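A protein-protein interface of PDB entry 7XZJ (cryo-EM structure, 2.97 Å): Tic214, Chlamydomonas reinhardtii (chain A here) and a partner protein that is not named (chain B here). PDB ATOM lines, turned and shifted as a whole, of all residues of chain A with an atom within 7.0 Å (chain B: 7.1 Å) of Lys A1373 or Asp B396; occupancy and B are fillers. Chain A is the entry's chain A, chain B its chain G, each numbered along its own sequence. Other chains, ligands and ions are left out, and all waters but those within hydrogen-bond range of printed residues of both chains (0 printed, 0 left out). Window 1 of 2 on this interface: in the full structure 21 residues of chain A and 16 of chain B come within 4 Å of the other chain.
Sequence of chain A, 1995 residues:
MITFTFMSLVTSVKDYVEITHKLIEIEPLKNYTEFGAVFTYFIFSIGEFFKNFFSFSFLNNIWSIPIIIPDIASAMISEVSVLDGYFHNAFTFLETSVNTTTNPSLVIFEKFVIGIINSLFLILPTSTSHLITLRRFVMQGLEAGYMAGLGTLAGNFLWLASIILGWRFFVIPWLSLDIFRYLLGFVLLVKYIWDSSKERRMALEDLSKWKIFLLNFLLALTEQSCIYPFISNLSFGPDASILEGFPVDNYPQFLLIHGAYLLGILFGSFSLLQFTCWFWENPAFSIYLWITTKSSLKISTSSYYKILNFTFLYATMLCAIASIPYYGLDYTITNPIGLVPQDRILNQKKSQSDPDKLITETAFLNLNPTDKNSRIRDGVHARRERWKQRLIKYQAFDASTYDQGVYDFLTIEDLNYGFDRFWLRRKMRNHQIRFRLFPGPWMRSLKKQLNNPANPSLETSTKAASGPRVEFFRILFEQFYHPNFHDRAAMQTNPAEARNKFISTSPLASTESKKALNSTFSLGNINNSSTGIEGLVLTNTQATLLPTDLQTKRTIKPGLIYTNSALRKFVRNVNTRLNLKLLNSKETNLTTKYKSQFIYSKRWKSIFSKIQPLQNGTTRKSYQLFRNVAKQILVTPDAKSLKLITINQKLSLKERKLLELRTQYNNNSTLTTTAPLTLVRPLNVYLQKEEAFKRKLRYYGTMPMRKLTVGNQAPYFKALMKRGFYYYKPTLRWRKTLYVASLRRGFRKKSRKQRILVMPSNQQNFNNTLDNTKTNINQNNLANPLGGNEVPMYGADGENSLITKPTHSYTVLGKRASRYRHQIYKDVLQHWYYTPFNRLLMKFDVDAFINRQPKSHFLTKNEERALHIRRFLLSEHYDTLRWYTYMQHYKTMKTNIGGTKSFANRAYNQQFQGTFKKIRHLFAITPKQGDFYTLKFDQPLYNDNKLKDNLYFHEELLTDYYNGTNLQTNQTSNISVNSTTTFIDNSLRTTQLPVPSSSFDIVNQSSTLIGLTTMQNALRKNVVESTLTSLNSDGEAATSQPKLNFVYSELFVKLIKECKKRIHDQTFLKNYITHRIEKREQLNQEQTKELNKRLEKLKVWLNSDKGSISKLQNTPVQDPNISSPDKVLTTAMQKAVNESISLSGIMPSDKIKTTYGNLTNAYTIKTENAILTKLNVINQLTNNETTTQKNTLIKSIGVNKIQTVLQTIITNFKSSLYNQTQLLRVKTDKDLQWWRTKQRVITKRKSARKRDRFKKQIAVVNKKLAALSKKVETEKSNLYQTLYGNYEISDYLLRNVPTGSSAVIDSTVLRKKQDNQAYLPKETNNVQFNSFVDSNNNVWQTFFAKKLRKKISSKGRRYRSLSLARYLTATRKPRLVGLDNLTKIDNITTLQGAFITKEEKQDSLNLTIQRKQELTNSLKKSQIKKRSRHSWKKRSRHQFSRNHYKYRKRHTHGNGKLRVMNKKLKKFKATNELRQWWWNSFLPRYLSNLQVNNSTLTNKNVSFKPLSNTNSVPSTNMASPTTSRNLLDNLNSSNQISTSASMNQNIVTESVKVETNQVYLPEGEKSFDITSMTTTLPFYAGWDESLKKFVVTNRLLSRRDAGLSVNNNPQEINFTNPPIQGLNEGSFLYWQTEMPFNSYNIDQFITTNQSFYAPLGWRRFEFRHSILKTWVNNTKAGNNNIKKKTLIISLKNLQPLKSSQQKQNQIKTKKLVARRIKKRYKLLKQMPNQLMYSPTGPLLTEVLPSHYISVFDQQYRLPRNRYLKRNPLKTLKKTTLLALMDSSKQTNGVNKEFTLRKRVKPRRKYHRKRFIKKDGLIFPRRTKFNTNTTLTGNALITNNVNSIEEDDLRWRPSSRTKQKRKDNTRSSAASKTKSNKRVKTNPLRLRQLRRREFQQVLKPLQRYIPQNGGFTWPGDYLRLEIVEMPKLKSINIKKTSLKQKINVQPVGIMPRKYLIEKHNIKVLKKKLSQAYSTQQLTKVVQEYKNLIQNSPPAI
N of Asp B396 sits at hydrogen-bond distance from O of Thr A1371 (3.2 Å). The guanidinium group (NH1) of Arg A1375 is in salt-bridge range of the side-chain carboxylate (OD1) of Asp B396, at 3.0 Å. O of Tyr B394 is in hydrogen-bond range of NZ of Lys A1433, at 3.1 Å.
O of Ala A1370 is in hydrogen-bond range of NH1 of Arg A1372 (3.3 Å). NH2 of Arg A1372 lies within salt-bridge range of OD1 of Asp A1386 (3.1 Å). O of Lys A1373 sits at hydrogen-bond distance from NH1 of Arg A1375, 2.8 Å away. The backbone carbonyl oxygen (O) of Arg A1375 lies within hydrogen-bond range of the backbone NH (N) of Lys A1384 (3.0 Å). The guanidinium group (NH2) of Arg A1429 sits at hydrogen-bond distance from a ring nitrogen (NE2) of His A1430, at 3.2 Å.
Asp B395 touches Ala A1370. CG2 of Thr A1371 touches O of Met B393 (3.6 Å). CD1 of Tyr B394 touches CG2 of Thr A1371, at 3.8 Å. N of Thr A1371 touches OD2 of Asp B395 (3.6 Å). Tyr B394 touches Arg A1372 (CE1 to O, 3.4 Å). Tyr B394 touches Lys A1373. Lys A1373 touches Asp B396 (CB to OD1, 3.5 Å). ND1 of His A1430 touches O of Glu B391 (3.6 Å). Tyr B394 touches His A1430. Lys A1433 touches Asp B395.
Lys A1373 touches just these residues of chain B: Tyr B394 and Asp B396. Of chain A, only Thr A1371 (3.2 Å), Lys A1373 (3.5 Å) and Arg A1375 (3.0 Å) come within 4 Å of Asp B396. Printed residues of chain B within 4 Å of Arg A1372: Tyr B394 (3.4 Å). Of the printed residues of chain B, Arg A1375 touches Asp B396. Ile A1385 touches none of the printed residues of chain B. The nearest residue of chain B that does not touch Lys A1373 is Glu B391 (5.1 Å).
Printed residues of chain A that touch a printed residue of chain B: Ala A1370, Thr A1371, Arg A1372, Lys A1373, Arg A1375, His A1430 and Lys A1433. Hydrophobic or aromatic side chains of chain A that line the printed part of chain B: Ala A1370 and His A1430. Hydrophobic or aromatic side chains of chain B within 4 Å of the printed part of chain A: Tyr B394. Among the printed residues, Asp or Glu carboxylates within 4 Å of a Lys or Arg side-chain nitrogen of the other chain: Arg A1375 with Asp B396.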
ATOM      1  N   ALA A1370     -25.660 -25.447  15.985  1.00  0.00           N
ATOM      2  CA  ALA A1370     -25.419 -23.984  16.033  1.00  0.00           C
ATOM      3  C   ALA A1370     -26.123 -23.294  14.857  1.00  0.00           C
ATOM      4  O   ALA A1370     -26.282 -23.944  13.805  1.00  0.00           O
ATOM      5  CB  ALA A1370     -23.937 -23.706  16.026  1.00  0.00           C
ATOM      6  N   THR A1371     -26.488 -22.018  15.020  1.00  0.00           N
ATOM      7  CA  THR A1371     -27.117 -21.243  13.915  1.00  0.00           C
ATOM      8  C   THR A1371     -26.020 -20.832  12.925  1.00  0.00           C
ATOM      9  O   THR A1371     -24.912 -20.500  13.389  1.00  0.00           O
ATOM     10  CB  THR A1371     -27.880 -20.033  14.468  1.00  0.00           C
ATOM     11  OG1 THR A1371     -28.591 -20.457  15.632  1.00  0.00           O
ATOM     12  CG2 THR A1371     -28.844 -19.429  13.471  1.00  0.00           C
ATOM     13  N   ARG A1372     -26.318 -20.846  11.621  1.00  0.00           N
ATOM     14  CA  ARG A1372     -25.292 -20.533  10.588  1.00  0.00           C
ATOM     15  C   ARG A1372     -25.766 -19.349   9.740  1.00  0.00           C
ATOM     16  O   ARG A1372     -26.986 -19.228   9.532  1.00  0.00           O
ATOM     17  CB  ARG A1372     -25.079 -21.736   9.667  1.00  0.00           C
ATOM     18  CG  ARG A1372     -24.507 -22.972  10.345  1.00  0.00           C
ATOM     19  CD  ARG A1372     -23.133 -22.741  10.943  1.00  0.00           C
ATOM     20  NE  ARG A1372     -22.314 -23.945  10.924  1.00  0.00           N
ATOM     21  CZ  ARG A1372     -22.353 -24.902  11.845  1.00  0.00           C
ATOM     22  NH1 ARG A1372     -23.184 -24.807  12.868  1.00  0.00           N
ATOM     23  NH2 ARG A1372     -21.564 -25.955  11.736  1.00  0.00           N
ATOM     24  N   LYS A1373     -24.838 -18.525   9.248  1.00  0.00           N
ATOM     25  CA  LYS A1373     -25.219 -17.381   8.376  1.00  0.00           C
ATOM     26  C   LYS A1373     -24.513 -17.503   7.024  1.00  0.00           C
ATOM     27  O   LYS A1373     -23.291 -17.266   6.977  1.00  0.00           O
ATOM     28  CB  LYS A1373     -24.866 -16.053   9.050  1.00  0.00           C
ATOM     29  CG  LYS A1373     -25.231 -14.807   8.256  1.00  0.00           C
ATOM     30  CD  LYS A1373     -24.674 -13.535   8.853  1.00  0.00           C
ATOM     31  CE  LYS A1373     -24.915 -12.324   7.978  1.00  0.00           C
ATOM     32  NZ  LYS A1373     -24.332 -12.501   6.627  1.00  0.00           N
ATOM     33  N   PRO A1374     -25.213 -17.859   5.924  1.00  0.00           N
ATOM     34  CA  PRO A1374     -24.579 -17.890   4.607  1.00  0.00           C
ATOM     35  C   PRO A1374     -24.141 -16.466   4.242  1.00  0.00           C
ATOM     36  O   PRO A1374     -24.936 -15.554   4.388  1.00  0.00           O
ATOM     37  CB  PRO A1374     -25.687 -18.384   3.665  1.00  0.00           C
ATOM     38  CG  PRO A1374     -26.979 -18.164   4.429  1.00  0.00           C
ATOM     39  CD  PRO A1374     -26.618 -18.266   5.895  1.00  0.00           C
ATOM     40  N   ARG A1375     -22.900 -16.308   3.778  1.00  0.00           N
ATOM     41  CA  ARG A1375     -22.382 -14.946   3.483  1.00  0.00           C
ATOM     42  C   ARG A1375     -21.380 -15.010   2.330  1.00  0.00           C
ATOM     43  O   ARG A1375     -20.736 -16.064   2.168  1.00  0.00           O
ATOM     44  CB  ARG A1375     -21.721 -14.371   4.739  1.00  0.00           C
ATOM     45  CG  ARG A1375     -20.638 -15.261   5.332  1.00  0.00           C
ATOM     46  CD  ARG A1375     -20.373 -14.982   6.798  1.00  0.00           C
ATOM     47  NE  ARG A1375     -19.298 -15.807   7.331  1.00  0.00           N
ATOM     48  CZ  ARG A1375     -19.464 -17.001   7.888  1.00  0.00           C
ATOM     49  NH1 ARG A1375     -20.674 -17.524   7.992  1.00  0.00           N
ATOM     50  NH2 ARG A1375     -18.419 -17.669   8.342  1.00  0.00           N
ATOM     51  N   LEU A1376     -21.263 -13.932   1.551  1.00  0.00           N
ATOM     52  CA  LEU A1376     -20.219 -13.898   0.495  1.00  0.00           C
ATOM     53  C   LEU A1376     -18.892 -13.676   1.226  1.00  0.00           C
ATOM     54  O   LEU A1376     -18.861 -12.820   2.129  1.00  0.00           O
ATOM     55  CB  LEU A1376     -20.509 -12.738  -0.463  1.00  0.00           C
ATOM     56  CG  LEU A1376     -19.833 -12.831  -1.830  1.00  0.00           C
ATOM     57  CD1 LEU A1376     -20.462 -13.933  -2.668  1.00  0.00           C
ATOM     58  CD2 LEU A1376     -19.916 -11.500  -2.562  1.00  0.00           C
ATOM     59  N   LYS A1384     -20.077 -18.981   1.812  1.00  0.00           N
ATOM     60  CA  LYS A1384     -19.695 -19.822   2.977  1.00  0.00           C
ATOM     61  C   LYS A1384     -20.828 -19.881   4.004  1.00  0.00           C
ATOM     62  O   LYS A1384     -21.169 -18.818   4.558  1.00  0.00           O
ATOM     63  CB  LYS A1384     -18.415 -19.286   3.626  1.00  0.00           C
ATOM     64  CG  LYS A1384     -17.946 -20.043   4.860  1.00  0.00           C
ATOM     65  CD  LYS A1384     -16.727 -19.428   5.507  1.00  0.00           C
ATOM     66  CE  LYS A1384     -16.217 -20.229   6.686  1.00  0.00           C
ATOM     67  NZ  LYS A1384     -15.792 -21.589   6.280  1.00  0.00           N
ATOM     68  N   ILE A1385     -21.389 -21.069   4.243  1.00  0.00           N
ATOM     69  CA  ILE A1385     -22.416 -21.229   5.314  1.00  0.00           C
ATOM     70  C   ILE A1385     -21.699 -21.964   6.448  1.00  0.00           C
ATOM     71  O   ILE A1385     -21.836 -21.536   7.612  1.00  0.00           O
ATOM     72  CB  ILE A1385     -23.668 -21.957   4.781  1.00  0.00           C
ATOM     73  CG1 ILE A1385     -24.794 -21.986   5.816  1.00  0.00           C
ATOM     74  CG2 ILE A1385     -23.323 -23.348   4.276  1.00  0.00           C
ATOM     75  CD1 ILE A1385     -26.128 -22.402   5.255  1.00  0.00           C
ATOM     76  N   ASP A1386     -20.938 -23.009   6.108  1.00  0.00           N
ATOM     77  CA  ASP A1386     -20.092 -23.699   7.119  1.00  0.00           C
ATOM     78  C   ASP A1386     -18.702 -23.884   6.501  1.00  0.00           C
ATOM     79  O   ASP A1386     -17.712 -23.847   7.258  1.00  0.00           O
ATOM     80  CB  ASP A1386     -20.721 -25.041   7.501  1.00  0.00           C
ATOM     81  CG  ASP A1386     -20.029 -25.722   8.668  1.00  0.00           C
ATOM     82  OD1 ASP A1386     -19.538 -25.002   9.559  1.00  0.00           O
ATOM     83  OD2 ASP A1386     -19.977 -26.966   8.672  1.00  0.00           O
ATOM     84  N   ARG A1429     -25.877  -6.044  20.081  1.00  0.00           N
ATOM     85  CA  ARG A1429     -25.979  -7.050  19.034  1.00  0.00           C
ATOM     86  C   ARG A1429     -26.257  -8.415  19.648  1.00  0.00           C
ATOM     87  O   ARG A1429     -25.716  -8.762  20.703  1.00  0.00           O
ATOM     88  CB  ARG A1429     -24.696  -7.092  18.205  1.00  0.00           C
ATOM     89  CG  ARG A1429     -23.448  -7.450  18.999  1.00  0.00           C
ATOM     90  CD  ARG A1429     -22.189  -7.256  18.171  1.00  0.00           C
ATOM     91  NE  ARG A1429     -22.085  -8.217  17.082  1.00  0.00           N
ATOM     92  CZ  ARG A1429     -21.413  -9.361  17.156  1.00  0.00           C
ATOM     93  NH1 ARG A1429     -20.784  -9.723  18.263  1.00  0.00           N
ATOM     94  NH2 ARG A1429     -21.370 -10.156  16.094  1.00  0.00           N
ATOM     95  N   HIS A1430     -27.114  -9.185  18.982  1.00  0.00           N
ATOM     96  CA  HIS A1430     -27.458 -10.538  19.410  1.00  0.00           C
ATOM     97  C   HIS A1430     -27.939 -10.553  20.859  1.00  0.00           C
ATOM     98  O   HIS A1430     -27.489 -11.351  21.684  1.00  0.00           O
ATOM     99  CB  HIS A1430     -26.278 -11.487  19.209  1.00  0.00           C
ATOM    100  CG  HIS A1430     -25.681 -11.425  17.836  1.00  0.00           C
ATOM    101  ND1 HIS A1430     -26.383 -11.778  16.704  1.00  0.00           N
ATOM    102  CD2 HIS A1430     -24.451 -11.052  17.414  1.00  0.00           C
ATOM    103  CE1 HIS A1430     -25.610 -11.623  15.643  1.00  0.00           C
ATOM    104  NE2 HIS A1430     -24.432 -11.184  16.047  1.00  0.00           N
ATOM    105  N   LYS A1433     -29.496 -13.801  21.938  1.00  0.00           N
ATOM    106  CA  LYS A1433     -28.497 -14.891  22.066  1.00  0.00           C
ATOM    107  C   LYS A1433     -27.797 -14.765  23.421  1.00  0.00           C
ATOM    108  O   LYS A1433     -27.700 -15.779  24.120  1.00  0.00           O
ATOM    109  CB  LYS A1433     -27.479 -14.811  20.926  1.00  0.00           C
ATOM    110  CG  LYS A1433     -26.522 -15.991  20.824  1.00  0.00           C
ATOM    111  CD  LYS A1433     -25.491 -15.825  19.731  1.00  0.00           C
ATOM    112  CE  LYS A1433     -24.532 -14.683  19.989  1.00  0.00           C
ATOM    113  NZ  LYS A1433     -23.603 -14.481  18.852  1.00  0.00           N
ATOM    114  N   GLU B 359     -27.647  -7.478  -1.656  1.00  0.00           N
ATOM    115  CA  GLU B 359     -26.475  -8.388  -1.544  1.00  0.00           C
ATOM    116  C   GLU B 359     -26.924  -9.746  -0.994  1.00  0.00           C
ATOM    117  O   GLU B 359     -26.450 -10.772  -1.511  1.00  0.00           O
ATOM    118  CB  GLU B 359     -25.399  -7.747  -0.665  1.00  0.00           C
ATOM    119  CG  GLU B 359     -24.197  -8.640  -0.408  1.00  0.00           C
ATOM    120  CD  GLU B 359     -24.194  -9.324   0.949  1.00  0.00           C
ATOM    121  OE1 GLU B 359     -25.083  -9.014   1.768  1.00  0.00           O
ATOM    122  OE2 GLU B 359     -23.303 -10.163   1.184  1.00  0.00           O
ATOM    123  N   GLU B 360     -27.812  -9.748   0.003  1.00  0.00           N
ATOM    124  CA  GLU B 360     -28.249 -11.022   0.634  1.00  0.00           C
ATOM    125  C   GLU B 360     -28.955 -11.880  -0.420  1.00  0.00           C
ATOM    126  O   GLU B 360     -28.693 -13.101  -0.464  1.00  0.00           O
ATOM    127  CB  GLU B 360     -29.171 -10.727   1.819  1.00  0.00           C
ATOM    128  CG  GLU B 360     -29.512 -11.949   2.653  1.00  0.00           C
ATOM    129  CD  GLU B 360     -30.846 -12.604   2.336  1.00  0.00           C
ATOM    130  OE1 GLU B 360     -31.554 -12.105   1.441  1.00  0.00           O
ATOM    131  OE2 GLU B 360     -31.176 -13.612   2.991  1.00  0.00           O
ATOM    132  N   GLU B 391     -31.938 -12.439  12.765  1.00  0.00           N
ATOM    133  CA  GLU B 391     -30.829 -11.461  12.922  1.00  0.00           C
ATOM    134  C   GLU B 391     -30.477 -11.324  14.408  1.00  0.00           C
ATOM    135  O   GLU B 391     -29.303 -11.027  14.708  1.00  0.00           O
ATOM    136  CB  GLU B 391     -31.199 -10.130  12.265  1.00  0.00           C
ATOM    137  CG  GLU B 391     -30.030  -9.171  12.146  1.00  0.00           C
ATOM    138  CD  GLU B 391     -28.834  -9.724  11.391  1.00  0.00           C
ATOM    139  OE1 GLU B 391     -29.039 -10.331  10.321  1.00  0.00           O
ATOM    140  OE2 GLU B 391     -27.700  -9.555  11.881  1.00  0.00           O
ATOM    141  N   MET B 393     -30.656 -13.870  16.719  1.00  0.00           N
ATOM    142  CA  MET B 393     -29.944 -15.087  17.187  1.00  0.00           C
ATOM    143  C   MET B 393     -29.044 -15.618  16.071  1.00  0.00           C
ATOM    144  O   MET B 393     -29.568 -16.287  15.163  1.00  0.00           O
ATOM    145  CB  MET B 393     -30.959 -16.162  17.585  1.00  0.00           C
ATOM    146  CG  MET B 393     -32.277 -16.041  16.845  1.00  0.00           C
ATOM    147  SD  MET B 393     -33.533 -17.178  17.479  1.00  0.00           S
ATOM    148  CE  MET B 393     -34.982 -16.581  16.612  1.00  0.00           C
ATOM    149  N   TYR B 394     -27.743 -15.326  16.142  1.00  0.00           N
ATOM    150  CA  TYR B 394     -26.791 -15.828  15.120  1.00  0.00           C
ATOM    151  C   TYR B 394     -25.478 -16.236  15.786  1.00  0.00           C
ATOM    152  O   TYR B 394     -24.648 -15.349  16.057  1.00  0.00           O
ATOM    153  CB  TYR B 394     -26.531 -14.773  14.043  1.00  0.00           C
ATOM    154  CG  TYR B 394     -27.325 -14.956  12.775  1.00  0.00           C
ATOM    155  CD1 TYR B 394     -27.348 -16.175  12.119  1.00  0.00           C
ATOM    156  CD2 TYR B 394     -28.040 -13.909  12.221  1.00  0.00           C
ATOM    157  CE1 TYR B 394     -28.073 -16.353  10.952  1.00  0.00           C
ATOM    158  CE2 TYR B 394     -28.768 -14.068  11.054  1.00  0.00           C
ATOM    159  CZ  TYR B 394     -28.782 -15.295  10.416  1.00  0.00           C
ATOM    160  OH  TYR B 394     -29.496 -15.461   9.265  1.00  0.00           O
ATOM    161  N   ASP B 395     -25.296 -17.536  16.031  1.00  0.00           N
ATOM    162  CA  ASP B 395     -24.004 -18.018  16.586  1.00  0.00           C
ATOM    163  C   ASP B 395     -22.923 -17.700  15.549  1.00  0.00           C
ATOM    164  O   ASP B 395     -21.827 -17.274  15.961  1.00  0.00           O
ATOM    165  CB  ASP B 395     -24.062 -19.510  16.924  1.00  0.00           C
ATOM    166  CG  ASP B 395     -25.155 -19.877  17.914  1.00  0.00           C
ATOM    167  OD1 ASP B 395     -25.901 -18.971  18.330  1.00  0.00           O
ATOM    168  OD2 ASP B 395     -25.250 -21.070  18.261  1.00  0.00           O
ATOM    169  N   ASP B 396     -23.233 -17.894  14.262  1.00  0.00           N
ATOM    170  CA  ASP B 396     -22.282 -17.562  13.167  1.00  0.00           C
ATOM    171  C   ASP B 396     -20.891 -18.104  13.514  1.00  0.00           C
ATOM    172  O   ASP B 396     -20.349 -18.849  12.675  1.00  0.00           O
ATOM    173  CB  ASP B 396     -22.271 -16.058  12.883  1.00  0.00           C
ATOM    174  CG  ASP B 396     -21.927 -15.714  11.445  1.00  0.00           C
ATOM    175  OD1 ASP B 396     -21.816 -16.651  10.632  1.00  0.00           O
ATOM    176  OD2 ASP B 396     -21.780 -14.512  11.148  1.00  0.00           O
